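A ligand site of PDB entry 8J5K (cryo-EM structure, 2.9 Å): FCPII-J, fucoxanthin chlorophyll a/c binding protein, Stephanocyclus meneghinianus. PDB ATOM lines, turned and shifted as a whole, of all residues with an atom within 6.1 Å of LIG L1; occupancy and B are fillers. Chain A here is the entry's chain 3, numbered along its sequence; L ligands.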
ATOM      1  N   LEU A   7      11.485 -15.409 -10.558  1.00  0.00           N
ATOM      2  CA  LEU A   7      11.520 -14.153  -9.829  1.00  0.00           C
ATOM      3  C   LEU A   7      10.726 -13.102 -10.612  1.00  0.00           C
ATOM      4  O   LEU A   7       9.949 -13.436 -11.508  1.00  0.00           O
ATOM      5  CB  LEU A   7      12.968 -13.701  -9.576  1.00  0.00           C
ATOM      6  N   ALA A   8      10.942 -11.837 -10.246  1.00  0.00           N
ATOM      7  CA  ALA A   8      10.196 -10.753 -10.858  1.00  0.00           C
ATOM      8  C   ALA A   8      10.453 -10.608 -12.354  1.00  0.00           C
ATOM      9  O   ALA A   8       9.518 -10.217 -13.085  1.00  0.00           O
ATOM     10  CB  ALA A   8      10.527  -9.450 -10.124  1.00  0.00           C
ATOM     11  N   PRO A   9      11.664 -10.840 -12.864  1.00  0.00           N
ATOM     12  CA  PRO A   9      11.873 -10.741 -14.324  1.00  0.00           C
ATOM     13  C   PRO A   9      10.973 -11.662 -15.135  1.00  0.00           C
ATOM     14  O   PRO A   9      10.458 -11.256 -16.181  1.00  0.00           O
ATOM     15  CB  PRO A   9      13.350 -11.129 -14.483  1.00  0.00           C
ATOM     16  N   THR A 120      17.892 -19.403  -4.365  1.00  0.00           N
ATOM     17  CA  THR A 120      17.402 -18.586  -5.486  1.00  0.00           C
ATOM     18  C   THR A 120      18.414 -17.511  -5.853  1.00  0.00           C
ATOM     19  O   THR A 120      18.702 -17.287  -7.041  1.00  0.00           O
ATOM     20  CB  THR A 120      16.068 -17.932  -5.116  1.00  0.00           C
ATOM     21  OG1 THR A 120      16.236 -17.162  -3.923  1.00  0.00           O
ATOM     22  CG2 THR A 120      14.988 -18.978  -4.920  1.00  0.00           C
ATOM     23  N   SER A 121      18.946 -16.818  -4.843  1.00  0.00           N
ATOM     24  CA  SER A 121      19.942 -15.777  -5.087  1.00  0.00           C
ATOM     25  C   SER A 121      21.180 -16.363  -5.764  1.00  0.00           C
ATOM     26  O   SER A 121      21.765 -15.731  -6.657  1.00  0.00           O
ATOM     27  CB  SER A 121      20.315 -15.112  -3.772  1.00  0.00           C
ATOM     28  OG  SER A 121      19.254 -14.298  -3.304  1.00  0.00           O
ATOM     29  N   GLU A 122      21.569 -17.566  -5.341  1.00  0.00           N
ATOM     30  CA  GLU A 122      22.688 -18.269  -5.964  1.00  0.00           C
ATOM     31  C   GLU A 122      22.447 -18.467  -7.446  1.00  0.00           C
ATOM     32  O   GLU A 122      23.302 -18.138  -8.282  1.00  0.00           O
ATOM     33  CB  GLU A 122      22.863 -19.636  -5.302  1.00  0.00           C
ATOM     34  N   GLN A 124      20.441 -16.948  -9.476  1.00  0.00           N
ATOM     35  CA  GLN A 124      20.437 -15.682 -10.204  1.00  0.00           C
ATOM     36  C   GLN A 124      21.856 -15.186 -10.455  1.00  0.00           C
ATOM     37  O   GLN A 124      22.205 -14.785 -11.570  1.00  0.00           O
ATOM     38  CB  GLN A 124      19.624 -14.646  -9.427  1.00  0.00           C
ATOM     39  N   HIS A 125      22.699 -15.232  -9.418  1.00  0.00           N
ATOM     40  CA  HIS A 125      24.061 -14.728  -9.546  1.00  0.00           C
ATOM     41  C   HIS A 125      24.867 -15.528 -10.561  1.00  0.00           C
ATOM     42  O   HIS A 125      25.599 -14.953 -11.376  1.00  0.00           O
ATOM     43  CB  HIS A 125      24.751 -14.767  -8.184  1.00  0.00           C
ATOM     44  CG  HIS A 125      24.467 -13.560  -7.362  1.00  0.00           C
ATOM     45  ND1 HIS A 125      23.479 -13.528  -6.411  1.00  0.00           N
ATOM     46  CD2 HIS A 125      25.013 -12.316  -7.393  1.00  0.00           C
ATOM     47  CE1 HIS A 125      23.445 -12.327  -5.852  1.00  0.00           C
ATOM     48  NE2 HIS A 125      24.364 -11.576  -6.444  1.00  0.00           N
ATOM     49  N   GLY A 126      24.766 -16.850 -10.502  1.00  0.00           N
ATOM     50  CA  GLY A 126      25.508 -17.681 -11.431  1.00  0.00           C
ATOM     51  C   GLY A 126      25.043 -17.488 -12.855  1.00  0.00           C
ATOM     52  O   GLY A 126      25.840 -17.492 -13.805  1.00  0.00           O
ATOM     53  N   LEU A 128      23.890 -14.695 -14.052  1.00  0.00           N
ATOM     54  CA  LEU A 128      24.498 -13.438 -14.468  1.00  0.00           C
ATOM     55  C   LEU A 128      25.968 -13.624 -14.832  1.00  0.00           C
ATOM     56  O   LEU A 128      26.469 -13.048 -15.807  1.00  0.00           O
ATOM     57  CB  LEU A 128      24.346 -12.408 -13.356  1.00  0.00           C
ATOM     58  CG  LEU A 128      24.647 -10.964 -13.745  1.00  0.00           C
ATOM     59  CD1 LEU A 128      23.924 -10.614 -15.024  1.00  0.00           C
ATOM     60  CD2 LEU A 128      24.234 -10.038 -12.621  1.00  0.00           C
HETATM   61 MG1  LIG L   1      17.026  -9.012  -9.923  1.00  0.00          MG
HETATM   62  C1  LIG L   1      17.426 -10.839  -6.996  1.00  0.00           C
HETATM   63  C2  LIG L   1      13.831  -8.260  -9.021  1.00  0.00           C
HETATM   64  C3  LIG L   1      16.731  -7.162 -12.788  1.00  0.00           C
HETATM   65  C4  LIG L   1      20.294  -9.951 -10.892  1.00  0.00           C
HETATM   66  N1  LIG L   1      15.850  -9.479  -8.252  1.00  0.00           N
HETATM   67  C5  LIG L   1      16.205 -10.252  -7.138  1.00  0.00           C
HETATM   68  C6  LIG L   1      15.040 -10.324  -6.143  1.00  0.00           C
HETATM   69  C7  LIG L   1      13.903  -9.548  -6.856  1.00  0.00           C
HETATM   70  C8  LIG L   1      14.564  -9.038  -8.140  1.00  0.00           C
HETATM   71  C9  LIG L   1      12.713 -10.426  -7.127  1.00  0.00           C
HETATM   72  C10 LIG L   1      15.363  -9.609  -4.849  1.00  0.00           C
HETATM   73  N2  LIG L   1      15.540  -7.967 -10.774  1.00  0.00           N
HETATM   74  C11 LIG L   1      14.315  -7.745 -10.237  1.00  0.00           C
HETATM   75  C12 LIG L   1      13.539  -6.849 -11.151  1.00  0.00           C
HETATM   76  C13 LIG L   1      14.348  -6.549 -12.202  1.00  0.00           C
HETATM   77  C14 LIG L   1      15.640  -7.231 -11.973  1.00  0.00           C
HETATM   78  C15 LIG L   1      12.180  -6.368 -10.890  1.00  0.00           C
HETATM   79  C16 LIG L   1      14.099  -5.702 -13.340  1.00  0.00           C
HETATM   80  N3  LIG L   1      18.307  -8.603 -11.516  1.00  0.00           N
HETATM   81  C17 LIG L   1      17.994  -7.778 -12.566  1.00  0.00           C
HETATM   82  C18 LIG L   1      19.128  -7.665 -13.471  1.00  0.00           C
HETATM   83  C19 LIG L   1      20.121  -8.504 -12.970  1.00  0.00           C
HETATM   84  C20 LIG L   1      19.588  -9.087 -11.742  1.00  0.00           C
HETATM   85  C21 LIG L   1      19.156  -6.845 -14.669  1.00  0.00           C
HETATM   86  N4  LIG L   1      18.582 -10.021  -9.134  1.00  0.00           N
HETATM   87  C22 LIG L   1      19.831 -10.396  -9.689  1.00  0.00           C
HETATM   88  C23 LIG L   1      20.528 -11.259  -8.725  1.00  0.00           C
HETATM   89  C24 LIG L   1      19.674 -11.417  -7.654  1.00  0.00           C
HETATM   90  C25 LIG L   1      18.455 -10.677  -7.981  1.00  0.00           C
HETATM   91  C26 LIG L   1      21.879 -11.771  -8.930  1.00  0.00           C
HETATM   92  C27 LIG L   1      19.487 -11.996  -6.338  1.00  0.00           C
HETATM   93  O1  LIG L   1      20.311 -12.534  -5.617  1.00  0.00           O
HETATM   94  C28 LIG L   1      17.995 -11.765  -5.951  1.00  0.00           C
HETATM   95  C1  LG2 L   2      22.833  -9.566 -29.329  1.00  0.00           C
HETATM   96  O1  LG2 L   2      20.915 -10.143 -16.850  1.00  0.00           O
HETATM   97  C2  LG2 L   2      23.287  -8.196 -28.893  1.00  0.00           C
HETATM   98  C3  LG2 L   2      20.934 -10.165 -20.087  1.00  0.00           C
HETATM   99  C4  LG2 L   2      20.708  -9.449 -18.993  1.00  0.00           C
HETATM  100  C5  LG2 L   2      21.046  -7.990 -18.954  1.00  0.00           C
HETATM  101  C6  LG2 L   2      20.155 -10.054 -17.795  1.00  0.00           C
HETATM  102  C7  LG2 L   2      18.724 -10.600 -17.759  1.00  0.00           C
HETATM  103  C8  LG2 L   2      18.486 -11.087 -16.373  1.00  0.00           C
HETATM  104  C9  LG2 L   2      18.063 -12.494 -15.889  1.00  0.00           C
HETATM  105  C10 LG2 L   2      17.862 -12.639 -14.362  1.00  0.00           C
HETATM  106  C11 LG2 L   2      17.712 -11.261 -13.711  1.00  0.00           C
HETATM  107  C12 LG2 L   2      16.727 -10.281 -14.393  1.00  0.00           C
HETATM  108  C13 LG2 L   2      23.111  -7.724 -27.654  1.00  0.00           C
HETATM  109  C14 LG2 L   2      17.276 -10.302 -15.833  1.00  0.00           C
HETATM  110  C15 LG2 L   2      16.614  -9.078 -16.559  1.00  0.00           C
HETATM  111  C16 LG2 L   2      18.831 -13.707 -16.385  1.00  0.00           C
HETATM  112  C17 LG2 L   2      16.789 -12.887 -16.645  1.00  0.00           C
HETATM  113  C18 LG2 L   2      23.898  -7.303 -29.887  1.00  0.00           C
HETATM  114  C19 LG2 L   2      24.123  -7.696 -31.135  1.00  0.00           C
HETATM  115  C20 LG2 L   2      24.732  -6.733 -32.028  1.00  0.00           C
HETATM  116  C21 LG2 L   2      25.027  -7.031 -33.300  1.00  0.00           C
HETATM  117  C22 LG2 L   2      24.645  -8.347 -33.882  1.00  0.00           C
HETATM  118  C23 LG2 L   2      25.641  -5.968 -34.119  1.00  0.00           C
HETATM  119  C24 LG2 L   2      22.546  -8.479 -26.541  1.00  0.00           C
HETATM  120  C25 LG2 L   2      26.068  -6.226 -35.263  1.00  0.00           C
HETATM  121  C26 LG2 L   2      26.536  -6.261 -36.431  1.00  0.00           C
HETATM  122  C27 LG2 L   2      25.943  -7.108 -37.520  1.00  0.00           C
HETATM  123  C28 LG2 L   2      26.449  -6.575 -38.842  1.00  0.00           C
HETATM  124  C29 LG2 L   2      27.000  -5.170 -38.791  1.00  0.00           C
HETATM  125  C30 LG2 L   2      28.240  -5.626 -38.044  1.00  0.00           C
HETATM  126  C31 LG2 L   2      27.904  -5.694 -36.559  1.00  0.00           C
HETATM  127  C32 LG2 L   2      28.873  -6.603 -35.835  1.00  0.00           C
HETATM  128  C33 LG2 L   2      28.205  -3.738 -40.246  1.00  0.00           C
HETATM  129  C34 LG2 L   2      29.551  -3.833 -40.893  1.00  0.00           C
HETATM  130  C35 LG2 L   2      22.320  -7.854 -25.374  1.00  0.00           C
HETATM  131  C36 LG2 L   2      24.549  -6.520 -37.378  1.00  0.00           C
HETATM  132  C37 LG2 L   2      26.027  -8.617 -37.318  1.00  0.00           C
HETATM  133  C38 LG2 L   2      21.782  -8.548 -24.194  1.00  0.00           C
HETATM  134  C39 LG2 L   2      22.433  -9.463 -23.469  1.00  0.00           C
HETATM  135  C40 LG2 L   2      23.881  -9.719 -23.670  1.00  0.00           C
HETATM  136  C41 LG2 L   2      21.832 -10.150 -22.310  1.00  0.00           C
HETATM  137  C42 LG2 L   2      21.507  -9.464 -21.227  1.00  0.00           C
HETATM  138  O2  LG2 L   2      18.597  -9.890 -15.536  1.00  0.00           O
HETATM  139  O3  LG2 L   2      17.343 -11.438 -12.333  1.00  0.00           O
HETATM  140  O4  LG2 L   2      27.968  -4.383 -35.975  1.00  0.00           O
HETATM  141  O5  LG2 L   2      27.311  -4.880 -40.158  1.00  0.00           O
HETATM  142  O6  LG2 L   2      27.785  -2.693 -39.771  1.00  0.00           O
HETATM  143 MG1  LG3 L   3      25.013  -9.436  -4.664  1.00  0.00          MG
HETATM  144  C1  LG3 L   3      22.324  -9.908  -2.519  1.00  0.00           C
HETATM  145  C2  LG3 L   3      26.952 -11.357  -2.646  1.00  0.00           C
HETATM  146  C3  LG3 L   3      27.569  -9.137  -6.926  1.00  0.00           C
HETATM  147  C4  LG3 L   3      22.905  -7.578  -6.812  1.00  0.00           C
HETATM  148  N1  LG3 L   3      24.682 -10.412  -2.848  1.00  0.00           N
HETATM  149  C5  LG3 L   3      23.493 -10.515  -2.120  1.00  0.00           C
HETATM  150  C6  LG3 L   3      23.691 -11.376  -0.859  1.00  0.00           C
HETATM  151  C7  LG3 L   3      25.187 -11.730  -0.908  1.00  0.00           C
HETATM  152  C8  LG3 L   3      25.657 -11.134  -2.229  1.00  0.00           C
HETATM  153  C9  LG3 L   3      25.945 -11.168   0.267  1.00  0.00           C
HETATM  154  C10 LG3 L   3      22.891 -12.664  -0.892  1.00  0.00           C
HETATM  155  N2  LG3 L   3      26.902 -10.123  -4.778  1.00  0.00           N
HETATM  156  C11 LG3 L   3      27.513 -10.863  -3.831  1.00  0.00           C
HETATM  157  C12 LG3 L   3      28.934 -11.071  -4.195  1.00  0.00           C
HETATM  158  C13 LG3 L   3      29.148 -10.456  -5.407  1.00  0.00           C
HETATM  159  C14 LG3 L   3      27.845  -9.834  -5.793  1.00  0.00           C
HETATM  160  C15 LG3 L   3      29.866 -11.838  -3.368  1.00  0.00           C
HETATM  161  C16 LG3 L   3      30.409 -10.443  -6.121  1.00  0.00           C
HETATM  162  C17 LG3 L   3      30.703 -10.013  -7.346  1.00  0.00           C
HETATM  163  N3  LG3 L   3      25.202  -8.485  -6.506  1.00  0.00           N
HETATM  164  C18 LG3 L   3      26.336  -8.501  -7.262  1.00  0.00           C
HETATM  165  C19 LG3 L   3      26.118  -7.784  -8.508  1.00  0.00           C
HETATM  166  C20 LG3 L   3      24.798  -7.331  -8.490  1.00  0.00           C
HETATM  167  C21 LG3 L   3      24.228  -7.791  -7.225  1.00  0.00           C
HETATM  168  C22 LG3 L   3      27.120  -7.608  -9.564  1.00  0.00           C
HETATM  169  N4  LG3 L   3      23.117  -8.752  -4.664  1.00  0.00           N
HETATM  170  C23 LG3 L   3      22.365  -8.026  -5.633  1.00  0.00           C
HETATM  171  C24 LG3 L   3      20.985  -7.857  -5.132  1.00  0.00           C
HETATM  172  C25 LG3 L   3      20.921  -8.539  -3.936  1.00  0.00           C
HETATM  173  C26 LG3 L   3      22.260  -9.114  -3.705  1.00  0.00           C
HETATM  174  C27 LG3 L   3      19.939  -7.116  -5.834  1.00  0.00           C
HETATM  175  C28 LG3 L   3      20.083  -8.924  -2.827  1.00  0.00           C
HETATM  176  O1  LG3 L   3      18.917  -8.637  -2.581  1.00  0.00           O
HETATM  177  C29 LG3 L   3      20.944  -9.862  -1.912  1.00  0.00           C
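The side-chain hydroxyl (OG) of Ser 121 is in hydrogen-bond range of an oxygen (O1) of LIG L1 (3.1 Å). An oxygen (O1) of LIG L1 sits close to a ring nitrogen (ND1) of His 125 (3.4 Å).
CB of Ala 8 touches C15 of LIG L1, at 3.6 Å. Gln 124 touches LIG L1. Hydrophobic or aromatic side chains within 4 Å of LIG L1: Ala 8 and His 125. Of the 10 residues printed, 4 come within 4 Å of LIG L1.
ND1 of His 125 is in hydrogen-bond range of O of Ser 121 (2.8 Å).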
